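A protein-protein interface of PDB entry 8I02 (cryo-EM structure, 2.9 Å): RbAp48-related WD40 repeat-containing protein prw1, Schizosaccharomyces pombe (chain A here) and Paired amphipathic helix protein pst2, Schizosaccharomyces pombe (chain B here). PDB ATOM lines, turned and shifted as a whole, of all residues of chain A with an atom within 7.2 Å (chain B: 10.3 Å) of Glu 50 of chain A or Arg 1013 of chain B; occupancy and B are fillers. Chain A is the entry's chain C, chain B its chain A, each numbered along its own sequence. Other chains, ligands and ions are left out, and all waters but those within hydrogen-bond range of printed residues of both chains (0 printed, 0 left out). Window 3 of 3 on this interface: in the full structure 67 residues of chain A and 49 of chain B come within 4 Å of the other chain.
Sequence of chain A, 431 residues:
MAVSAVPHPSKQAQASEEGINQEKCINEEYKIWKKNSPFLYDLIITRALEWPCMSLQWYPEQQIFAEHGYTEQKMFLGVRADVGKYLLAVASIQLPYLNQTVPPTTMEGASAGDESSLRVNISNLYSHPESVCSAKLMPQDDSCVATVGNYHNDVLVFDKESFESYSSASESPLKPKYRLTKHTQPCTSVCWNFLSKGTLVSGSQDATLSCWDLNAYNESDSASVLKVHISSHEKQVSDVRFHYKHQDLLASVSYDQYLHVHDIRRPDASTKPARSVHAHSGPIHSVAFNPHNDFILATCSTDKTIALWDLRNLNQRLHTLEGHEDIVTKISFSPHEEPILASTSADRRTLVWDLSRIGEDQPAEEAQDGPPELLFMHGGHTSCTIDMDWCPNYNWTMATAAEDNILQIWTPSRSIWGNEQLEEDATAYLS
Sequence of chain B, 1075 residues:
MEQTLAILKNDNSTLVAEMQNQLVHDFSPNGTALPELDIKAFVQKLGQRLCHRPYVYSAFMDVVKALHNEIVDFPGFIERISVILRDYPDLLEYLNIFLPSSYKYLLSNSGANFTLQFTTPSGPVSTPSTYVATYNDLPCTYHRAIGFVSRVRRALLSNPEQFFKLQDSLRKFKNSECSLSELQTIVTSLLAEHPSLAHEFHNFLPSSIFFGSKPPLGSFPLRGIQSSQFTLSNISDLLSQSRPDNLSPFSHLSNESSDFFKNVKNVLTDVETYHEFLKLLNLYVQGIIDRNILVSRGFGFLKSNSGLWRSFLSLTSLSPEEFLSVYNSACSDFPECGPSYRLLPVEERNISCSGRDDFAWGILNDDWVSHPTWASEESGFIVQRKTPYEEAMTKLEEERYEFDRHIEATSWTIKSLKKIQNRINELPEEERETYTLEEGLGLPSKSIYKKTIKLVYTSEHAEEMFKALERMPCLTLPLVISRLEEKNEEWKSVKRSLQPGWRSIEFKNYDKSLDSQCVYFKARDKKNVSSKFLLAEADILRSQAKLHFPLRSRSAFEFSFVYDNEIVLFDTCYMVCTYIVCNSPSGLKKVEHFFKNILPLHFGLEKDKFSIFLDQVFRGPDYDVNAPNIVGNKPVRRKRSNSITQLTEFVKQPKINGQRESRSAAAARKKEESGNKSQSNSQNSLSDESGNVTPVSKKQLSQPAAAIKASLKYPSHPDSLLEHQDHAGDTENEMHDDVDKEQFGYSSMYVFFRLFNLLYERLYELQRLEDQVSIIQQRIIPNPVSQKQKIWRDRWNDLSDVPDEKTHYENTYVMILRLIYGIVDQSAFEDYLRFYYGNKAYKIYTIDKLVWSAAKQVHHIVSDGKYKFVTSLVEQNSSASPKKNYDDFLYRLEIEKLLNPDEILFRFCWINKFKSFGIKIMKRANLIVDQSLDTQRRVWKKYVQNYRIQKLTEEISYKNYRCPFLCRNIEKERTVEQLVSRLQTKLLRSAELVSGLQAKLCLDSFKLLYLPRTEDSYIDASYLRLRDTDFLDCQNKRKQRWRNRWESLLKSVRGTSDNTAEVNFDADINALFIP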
ATOM      1  N   ARG A  47      -5.900 -18.092   3.378  1.00  0.00           N
ATOM      2  CA  ARG A  47      -5.580 -16.724   3.768  1.00  0.00           C
ATOM      3  C   ARG A  47      -6.826 -15.874   3.577  1.00  0.00           C
ATOM      4  O   ARG A  47      -7.203 -15.569   2.443  1.00  0.00           O
ATOM      5  CB  ARG A  47      -4.415 -16.181   2.945  1.00  0.00           C
ATOM      6  CG  ARG A  47      -4.038 -14.738   3.256  1.00  0.00           C
ATOM      7  CD  ARG A  47      -2.887 -14.647   4.248  1.00  0.00           C
ATOM      8  NE  ARG A  47      -2.450 -13.265   4.444  1.00  0.00           N
ATOM      9  CZ  ARG A  47      -1.451 -12.892   5.242  1.00  0.00           C
ATOM     10  NH1 ARG A  47      -0.766 -13.792   5.935  1.00  0.00           N
ATOM     11  NH2 ARG A  47      -1.135 -11.613   5.346  1.00  0.00           N
ATOM     12  N   ALA A  48      -7.463 -15.504   4.684  1.00  0.00           N
ATOM     13  CA  ALA A  48      -8.667 -14.689   4.614  1.00  0.00           C
ATOM     14  C   ALA A  48      -8.344 -13.330   4.014  1.00  0.00           C
ATOM     15  O   ALA A  48      -7.415 -12.648   4.454  1.00  0.00           O
ATOM     16  CB  ALA A  48      -9.276 -14.530   6.003  1.00  0.00           C
ATOM     17  N   LEU A  49      -9.107 -12.940   3.005  1.00  0.00           N
ATOM     18  CA  LEU A  49      -8.817 -11.740   2.245  1.00  0.00           C
ATOM     19  C   LEU A  49      -9.616 -10.559   2.786  1.00  0.00           C
ATOM     20  O   LEU A  49     -10.271 -10.639   3.830  1.00  0.00           O
ATOM     21  CB  LEU A  49      -9.097 -11.985   0.763  1.00  0.00           C
ATOM     22  CG  LEU A  49      -7.858 -12.028  -0.126  1.00  0.00           C
ATOM     23  CD1 LEU A  49      -6.831 -12.991   0.438  1.00  0.00           C
ATOM     24  CD2 LEU A  49      -8.233 -12.410  -1.542  1.00  0.00           C
ATOM     25  N   GLU A  50      -9.556  -9.438   2.066  1.00  0.00           N
ATOM     26  CA  GLU A  50     -10.251  -8.218   2.449  1.00  0.00           C
ATOM     27  C   GLU A  50     -11.516  -7.969   1.639  1.00  0.00           C
ATOM     28  O   GLU A  50     -12.418  -7.279   2.127  1.00  0.00           O
ATOM     29  CB  GLU A  50      -9.321  -7.008   2.290  1.00  0.00           C
ATOM     30  CG  GLU A  50      -8.211  -6.875   3.335  1.00  0.00           C
ATOM     31  CD  GLU A  50      -6.991  -7.736   3.032  1.00  0.00           C
ATOM     32  OE1 GLU A  50      -7.145  -8.955   2.814  1.00  0.00           O
ATOM     33  OE2 GLU A  50      -5.870  -7.187   3.002  1.00  0.00           O
ATOM     34  N   TRP A  51     -11.604  -8.506   0.430  1.00  0.00           N
ATOM     35  CA  TRP A  51     -12.706  -8.257  -0.483  1.00  0.00           C
ATOM     36  C   TRP A  51     -13.001  -9.524  -1.268  1.00  0.00           C
ATOM     37  O   TRP A  51     -12.154 -10.420  -1.353  1.00  0.00           O
ATOM     38  CB  TRP A  51     -12.373  -7.117  -1.455  1.00  0.00           C
ATOM     39  CG  TRP A  51     -11.301  -6.192  -0.970  1.00  0.00           C
ATOM     40  CD1 TRP A  51      -9.961  -6.295  -1.207  1.00  0.00           C
ATOM     41  CD2 TRP A  51     -11.478  -5.024  -0.162  1.00  0.00           C
ATOM     42  NE1 TRP A  51      -9.293  -5.261  -0.599  1.00  0.00           N
ATOM     43  CE2 TRP A  51     -10.201  -4.467   0.049  1.00  0.00           C
ATOM     44  CE3 TRP A  51     -12.590  -4.394   0.405  1.00  0.00           C
ATOM     45  CZ2 TRP A  51     -10.008  -3.310   0.802  1.00  0.00           C
ATOM     46  CZ3 TRP A  51     -12.396  -3.247   1.149  1.00  0.00           C
ATOM     47  CH2 TRP A  51     -11.114  -2.717   1.342  1.00  0.00           C
ATOM     48  N   PRO A  52     -14.195  -9.630  -1.856  1.00  0.00           N
ATOM     49  CA  PRO A  52     -14.472 -10.756  -2.756  1.00  0.00           C
ATOM     50  C   PRO A  52     -13.545 -10.747  -3.957  1.00  0.00           C
ATOM     51  O   PRO A  52     -13.176  -9.694  -4.473  1.00  0.00           O
ATOM     52  CB  PRO A  52     -15.926 -10.522  -3.182  1.00  0.00           C
ATOM     53  CG  PRO A  52     -16.503  -9.683  -2.119  1.00  0.00           C
ATOM     54  CD  PRO A  52     -15.393  -8.806  -1.627  1.00  0.00           C
ATOM     55  N   VAL A  79     -10.811  -7.822  -7.524  1.00  0.00           N
ATOM     56  CA  VAL A  79     -11.653  -7.713  -6.341  1.00  0.00           C
ATOM     57  C   VAL A  79     -12.834  -6.804  -6.657  1.00  0.00           C
ATOM     58  O   VAL A  79     -12.914  -6.197  -7.725  1.00  0.00           O
ATOM     59  CB  VAL A  79     -10.869  -7.202  -5.115  1.00  0.00           C
ATOM     60  CG1 VAL A  79     -10.303  -8.361  -4.336  1.00  0.00           C
ATOM     61  CG2 VAL A  79      -9.737  -6.328  -5.560  1.00  0.00           C
ATOM     62  N   ALA A  81     -14.189  -4.461  -4.080  1.00  0.00           N
ATOM     63  CA  ALA A  81     -14.106  -3.876  -2.744  1.00  0.00           C
ATOM     64  C   ALA A  81     -15.414  -3.264  -2.261  1.00  0.00           C
ATOM     65  O   ALA A  81     -15.749  -3.369  -1.078  1.00  0.00           O
ATOM     66  CB  ALA A  81     -12.999  -2.823  -2.708  1.00  0.00           C
ATOM     67  N   ARG A 119       2.798 -17.676   4.276  1.00  0.00           N
ATOM     68  CA  ARG A 119       1.718 -16.719   4.111  1.00  0.00           C
ATOM     69  C   ARG A 119       1.462 -16.427   2.637  1.00  0.00           C
ATOM     70  O   ARG A 119       2.229 -16.799   1.746  1.00  0.00           O
ATOM     71  CB  ARG A 119       2.037 -15.417   4.849  1.00  0.00           C
ATOM     72  CG  ARG A 119       2.346 -15.574   6.323  1.00  0.00           C
ATOM     73  CD  ARG A 119       3.699 -14.972   6.643  1.00  0.00           C
ATOM     74  NE  ARG A 119       3.905 -14.788   8.076  1.00  0.00           N
ATOM     75  CZ  ARG A 119       4.984 -14.223   8.606  1.00  0.00           C
ATOM     76  NH1 ARG A 119       5.958 -13.790   7.820  1.00  0.00           N
ATOM     77  NH2 ARG A 119       5.090 -14.090   9.920  1.00  0.00           N
ATOM     78  N   VAL A 120       0.342 -15.756   2.396  1.00  0.00           N
ATOM     79  CA  VAL A 120      -0.004 -15.204   1.096  1.00  0.00           C
ATOM     80  C   VAL A 120      -0.052 -13.697   1.295  1.00  0.00           C
ATOM     81  O   VAL A 120      -0.989 -13.174   1.912  1.00  0.00           O
ATOM     82  CB  VAL A 120      -1.338 -15.745   0.568  1.00  0.00           C
ATOM     83  CG1 VAL A 120      -1.724 -15.033  -0.714  1.00  0.00           C
ATOM     84  CG2 VAL A 120      -1.256 -17.246   0.348  1.00  0.00           C
ATOM     85  N   ILE A 122      -0.292  -9.802   0.117  1.00  0.00           N
ATOM     86  CA  ILE A 122      -0.827  -8.952  -0.939  1.00  0.00           C
ATOM     87  C   ILE A 122       0.210  -7.900  -1.307  1.00  0.00           C
ATOM     88  O   ILE A 122       0.836  -7.285  -0.436  1.00  0.00           O
ATOM     89  CB  ILE A 122      -2.159  -8.316  -0.506  1.00  0.00           C
ATOM     90  CG1 ILE A 122      -3.328  -9.228  -0.881  1.00  0.00           C
ATOM     91  CG2 ILE A 122      -2.353  -6.954  -1.157  1.00  0.00           C
ATOM     92  CD1 ILE A 122      -3.519  -9.400  -2.377  1.00  0.00           C
ATOM     93  N   ASN A 405     -14.757 -13.888   1.118  1.00  0.00           N
ATOM     94  CA  ASN A 405     -13.443 -13.282   1.341  1.00  0.00           C
ATOM     95  C   ASN A 405     -12.406 -14.327   1.762  1.00  0.00           C
ATOM     96  O   ASN A 405     -11.694 -14.153   2.750  1.00  0.00           O
ATOM     97  CB  ASN A 405     -13.521 -12.152   2.371  1.00  0.00           C
ATOM     98  CG  ASN A 405     -14.742 -11.272   2.187  1.00  0.00           C
ATOM     99  OD1 ASN A 405     -15.420 -10.924   3.153  1.00  0.00           O
ATOM    100  ND2 ASN A 405     -15.026 -10.903   0.945  1.00  0.00           N
ATOM    101  N   ILE A 406     -12.314 -15.411   0.992  1.00  0.00           N
ATOM    102  CA  ILE A 406     -11.359 -16.481   1.252  1.00  0.00           C
ATOM    103  C   ILE A 406     -10.636 -16.812  -0.045  1.00  0.00           C
ATOM    104  O   ILE A 406     -11.113 -16.522  -1.142  1.00  0.00           O
ATOM    105  CB  ILE A 406     -12.031 -17.749   1.828  1.00  0.00           C
ATOM    106  CG1 ILE A 406     -13.016 -17.390   2.935  1.00  0.00           C
ATOM    107  CG2 ILE A 406     -10.999 -18.715   2.390  1.00  0.00           C
ATOM    108  CD1 ILE A 406     -12.352 -17.010   4.224  1.00  0.00           C
ATOM    109  N   VAL B 994      -0.185 -24.241  11.443  1.00  0.00           N
ATOM    110  CA  VAL B 994      -0.427 -22.849  11.796  1.00  0.00           C
ATOM    111  C   VAL B 994      -1.930 -22.638  11.819  1.00  0.00           C
ATOM    112  O   VAL B 994      -2.639 -23.143  10.945  1.00  0.00           O
ATOM    113  CB  VAL B 994       0.245 -21.897  10.786  1.00  0.00           C
ATOM    114  CG1 VAL B 994      -0.322 -20.491  10.895  1.00  0.00           C
ATOM    115  CG2 VAL B 994       1.757 -21.907  10.975  1.00  0.00           C
ATOM    116  N   SER B 995      -2.426 -21.922  12.822  1.00  0.00           N
ATOM    117  CA  SER B 995      -3.864 -21.728  12.946  1.00  0.00           C
ATOM    118  C   SER B 995      -4.218 -20.292  13.285  1.00  0.00           C
ATOM    119  O   SER B 995      -5.004 -20.032  14.197  1.00  0.00           O
ATOM    120  CB  SER B 995      -4.460 -22.663  13.988  1.00  0.00           C
ATOM    121  OG  SER B 995      -5.590 -22.057  14.577  1.00  0.00           O
ATOM    122  N   GLY B 996      -3.653 -19.330  12.560  1.00  0.00           N
ATOM    123  CA  GLY B 996      -3.942 -17.937  12.861  1.00  0.00           C
ATOM    124  C   GLY B 996      -5.394 -17.566  12.619  1.00  0.00           C
ATOM    125  O   GLY B 996      -5.962 -16.748  13.345  1.00  0.00           O
ATOM    126  N   LEU B 997      -6.007 -18.165  11.604  1.00  0.00           N
ATOM    127  CA  LEU B 997      -7.336 -17.805  11.124  1.00  0.00           C
ATOM    128  C   LEU B 997      -8.366 -17.735  12.240  1.00  0.00           C
ATOM    129  O   LEU B 997      -8.536 -18.685  13.008  1.00  0.00           O
ATOM    130  CB  LEU B 997      -7.783 -18.817  10.070  1.00  0.00           C
ATOM    131  CG  LEU B 997      -9.155 -18.583   9.441  1.00  0.00           C
ATOM    132  CD1 LEU B 997      -9.030 -17.783   8.163  1.00  0.00           C
ATOM    133  CD2 LEU B 997      -9.824 -19.903   9.166  1.00  0.00           C
ATOM    134  N   GLN B 998      -9.060 -16.600  12.321  1.00  0.00           N
ATOM    135  CA  GLN B 998     -10.209 -16.413  13.196  1.00  0.00           C
ATOM    136  C   GLN B 998     -11.361 -15.845  12.381  1.00  0.00           C
ATOM    137  O   GLN B 998     -11.212 -15.515  11.203  1.00  0.00           O
ATOM    138  CB  GLN B 998      -9.888 -15.485  14.375  1.00  0.00           C
ATOM    139  CG  GLN B 998      -9.598 -14.059  13.983  1.00  0.00           C
ATOM    140  CD  GLN B 998      -9.917 -13.075  15.088  1.00  0.00           C
ATOM    141  OE1 GLN B 998     -10.748 -13.347  15.955  1.00  0.00           O
ATOM    142  NE2 GLN B 998      -9.266 -11.919  15.057  1.00  0.00           N
ATOM    143  N   ALA B 999     -12.520 -15.730  13.013  1.00  0.00           N
ATOM    144  CA  ALA B 999     -13.706 -15.230  12.334  1.00  0.00           C
ATOM    145  C   ALA B 999     -14.682 -14.712  13.379  1.00  0.00           C
ATOM    146  O   ALA B 999     -14.328 -14.535  14.549  1.00  0.00           O
ATOM    147  CB  ALA B 999     -14.335 -16.317  11.458  1.00  0.00           C
ATOM    148  N   LEU B1009     -17.745 -14.516   9.293  1.00  0.00           N
ATOM    149  CA  LEU B1009     -17.055 -13.334   8.782  1.00  0.00           C
ATOM    150  C   LEU B1009     -15.587 -13.473   9.160  1.00  0.00           C
ATOM    151  O   LEU B1009     -15.206 -13.184  10.298  1.00  0.00           O
ATOM    152  CB  LEU B1009     -17.641 -12.048   9.351  1.00  0.00           C
ATOM    153  CG  LEU B1009     -19.122 -11.719   9.170  1.00  0.00           C
ATOM    154  CD1 LEU B1009     -19.625 -12.128   7.793  1.00  0.00           C
ATOM    155  CD2 LEU B1009     -19.933 -12.369  10.266  1.00  0.00           C
ATOM    156  N   TYR B1010     -14.764 -13.909   8.215  1.00  0.00           N
ATOM    157  CA  TYR B1010     -13.349 -14.133   8.489  1.00  0.00           C
ATOM    158  C   TYR B1010     -12.623 -12.793   8.534  1.00  0.00           C
ATOM    159  O   TYR B1010     -12.537 -12.092   7.524  1.00  0.00           O
ATOM    160  CB  TYR B1010     -12.751 -15.046   7.424  1.00  0.00           C
ATOM    161  CG  TYR B1010     -13.273 -16.464   7.467  1.00  0.00           C
ATOM    162  CD1 TYR B1010     -12.491 -17.497   7.959  1.00  0.00           C
ATOM    163  CD2 TYR B1010     -14.546 -16.770   7.013  1.00  0.00           C
ATOM    164  CE1 TYR B1010     -12.961 -18.787   7.994  1.00  0.00           C
ATOM    165  CE2 TYR B1010     -15.024 -18.057   7.052  1.00  0.00           C
ATOM    166  CZ  TYR B1010     -14.226 -19.059   7.544  1.00  0.00           C
ATOM    167  OH  TYR B1010     -14.697 -20.344   7.581  1.00  0.00           O
ATOM    168  N   LEU B1011     -12.103 -12.439   9.700  1.00  0.00           N
ATOM    169  CA  LEU B1011     -11.417 -11.163   9.853  1.00  0.00           C
ATOM    170  C   LEU B1011     -10.113 -11.170   9.062  1.00  0.00           C
ATOM    171  O   LEU B1011      -9.329 -12.119   9.174  1.00  0.00           O
ATOM    172  CB  LEU B1011     -11.156 -10.867  11.326  1.00  0.00           C
ATOM    173  CG  LEU B1011     -12.371 -10.937  12.255  1.00  0.00           C
ATOM    174  CD1 LEU B1011     -12.111 -10.137  13.513  1.00  0.00           C
ATOM    175  CD2 LEU B1011     -13.629 -10.429  11.574  1.00  0.00           C
ATOM    176  N   PRO B1012      -9.841 -10.132   8.271  1.00  0.00           N
ATOM    177  CA  PRO B1012      -8.766 -10.211   7.273  1.00  0.00           C
ATOM    178  C   PRO B1012      -7.389 -10.320   7.907  1.00  0.00           C
ATOM    179  O   PRO B1012      -7.223 -10.134   9.111  1.00  0.00           O
ATOM    180  CB  PRO B1012      -8.918  -8.904   6.487  1.00  0.00           C
ATOM    181  CG  PRO B1012     -10.321  -8.455   6.759  1.00  0.00           C
ATOM    182  CD  PRO B1012     -10.589  -8.870   8.167  1.00  0.00           C
ATOM    183  N   ARG B1013      -6.403 -10.646   7.073  1.00  0.00           N
ATOM    184  CA  ARG B1013      -4.987 -10.809   7.382  1.00  0.00           C
ATOM    185  C   ARG B1013      -4.712 -12.087   8.161  1.00  0.00           C
ATOM    186  O   ARG B1013      -3.546 -12.396   8.408  1.00  0.00           O
ATOM    187  CB  ARG B1013      -4.390  -9.621   8.162  1.00  0.00           C
ATOM    188  CG  ARG B1013      -3.073  -9.103   7.609  1.00  0.00           C
ATOM    189  CD  ARG B1013      -3.281  -8.346   6.311  1.00  0.00           C
ATOM    190  NE  ARG B1013      -4.485  -7.523   6.351  1.00  0.00           N
ATOM    191  CZ  ARG B1013      -4.568  -6.346   6.959  1.00  0.00           C
ATOM    192  NH1 ARG B1013      -3.513  -5.841   7.577  1.00  0.00           N
ATOM    193  NH2 ARG B1013      -5.707  -5.672   6.944  1.00  0.00           N
ATOM    194  N   THR B1014      -5.728 -12.846   8.552  1.00  0.00           N
ATOM    195  CA  THR B1014      -5.548 -14.064   9.326  1.00  0.00           C
ATOM    196  C   THR B1014      -5.588 -15.265   8.392  1.00  0.00           C
ATOM    197  O   THR B1014      -6.456 -15.341   7.516  1.00  0.00           O
ATOM    198  CB  THR B1014      -6.632 -14.187  10.395  1.00  0.00           C
ATOM    199  OG1 THR B1014      -7.920 -14.081   9.781  1.00  0.00           O
ATOM    200  CG2 THR B1014      -6.477 -13.091  11.434  1.00  0.00           C
ATOM    201  N   GLU B1015      -4.647 -16.190   8.573  1.00  0.00           N
ATOM    202  CA  GLU B1015      -4.564 -17.368   7.725  1.00  0.00           C
ATOM    203  C   GLU B1015      -4.294 -18.603   8.569  1.00  0.00           C
ATOM    204  O   GLU B1015      -3.863 -18.517   9.718  1.00  0.00           O
ATOM    205  CB  GLU B1015      -3.472 -17.236   6.664  1.00  0.00           C
ATOM    206  CG  GLU B1015      -2.104 -17.668   7.129  1.00  0.00           C
ATOM    207  CD  GLU B1015      -1.227 -18.121   5.984  1.00  0.00           C
ATOM    208  OE1 GLU B1015      -0.393 -19.026   6.188  1.00  0.00           O
ATOM    209  OE2 GLU B1015      -1.379 -17.575   4.874  1.00  0.00           O
ATOM    210  N   ASP B1016      -4.552 -19.761   7.966  1.00  0.00           N
ATOM    211  CA  ASP B1016      -4.294 -21.068   8.555  1.00  0.00           C
ATOM    212  C   ASP B1016      -3.532 -21.903   7.538  1.00  0.00           C
ATOM    213  O   ASP B1016      -3.767 -21.780   6.335  1.00  0.00           O
ATOM    214  CB  ASP B1016      -5.601 -21.762   8.943  1.00  0.00           C
ATOM    215  CG  ASP B1016      -5.385 -22.991   9.807  1.00  0.00           C
ATOM    216  OD1 ASP B1016      -5.866 -22.995  10.959  1.00  0.00           O
ATOM    217  OD2 ASP B1016      -4.744 -23.956   9.340  1.00  0.00           O
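O of Thr 1014 of chain B lies within hydrogen-bond range of N of Ala 48 of chain A.
The guanidinium group of Arg 1013 of chain B is in salt-bridge range of the side-chain carboxylate of Glu 50 of chain A (3.6 Å).
The backbone NH of Arg 1013 of chain B lies within hydrogen-bond range of the backbone carbonyl oxygen of Ala 48 of chain A (3.4 Å).
The side-chain carboxylate of Glu 1015 of chain B lies within salt-bridge range of the guanidinium group of Arg 47 of chain A (3.98 Å).
N of Gly 996 of chain B lies within hydrogen-bond range of O of Glu 1015 of chain B, 3.0 Å away.
The guanidinium group of Arg 47 of chain A lies within hydrogen-bond range of the backbone carbonyl oxygen of Val 120 of chain A (2.9 Å).
The backbone carbonyl oxygen (O) of Leu 1011 of chain B is in hydrogen-bond range of the side-chain hydroxyl (OG1) of Thr 1014 of chain B (2.5 Å).
O of Asn 405 of chain A lies within hydrogen-bond range of N of Leu 49 of chain A, 2.9 Å away.
The backbone NH (N) of Leu 997 of chain B sits at hydrogen-bond distance from the backbone carbonyl oxygen (O) of Glu 1015 of chain B (2.9 Å).
Among the printed residues, pairs that only touch across the chains: Arg 119 of chain A with Glu 1015 of chain B, Ile 406 of chain A with Tyr 1010 of chain B, Leu 49 of chain A with Pro 1012 of chain B, Val 120 of chain A with Glu 1015 of chain B, Ala 48 of chain A with Tyr 1010 of chain B, Glu 50 of chain A with Pro 1012 of chain B, Arg 47 of chain A with Arg 1013 of chain B, Ala 48 of chain A with Leu 997 of chain B, Ala 48 of chain A with Pro 1012 of chain B, Ala 48 of chain A with Leu 1011 of chain B and Arg 47 of chain A with Thr 1014 of chain B.
Of the printed residues of chain B, Arg 47 of chain A touches Arg 1013 (3.8 Å), Thr 1014 (3.99 Å) and Glu 1015 (3.4 Å).
Leu 49 of chain A touches just one residue of chain B: Pro 1012 (3.4 Å).
Of chain B, only Pro 1012 (3.8 Å) and Arg 1013 (3.6 Å) come within 4 Å of Glu 50 of chain A.
Pro 52 of chain A touches none of the printed residues of chain B.
Gly 996 of chain B touches none of the printed residues of chain A.
Of the printed residues of chain A, Pro 1012 of chain B touches Ala 48, Leu 49 and Glu 50.
Arg 1013 of chain B touches just these residues of chain A: Arg 47, Ala 48 and Glu 50.
Printed residues of chain B that touch a printed residue of chain A: Leu 997, Tyr 1010, Leu 1011, Pro 1012, Arg 1013, Thr 1014 and Glu 1015.
Hydrophobic or aromatic side chains of chain B within 4 Å of the printed part of chain A: Leu 997, Tyr 1010 and Pro 1012.
Along chain B the printed residues that touch a printed residue of chain A span positions 997 to 1015.
Among the printed residues, 15 pairs touch across the chains.
Among the printed residues, Asp or Glu carboxylates within 4 Å of a Lys or Arg side-chain nitrogen of the other chain: Arg 47 of chain A with Glu 1015 of chain B and Glu 50 of chain A with Arg 1013 of chain B.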
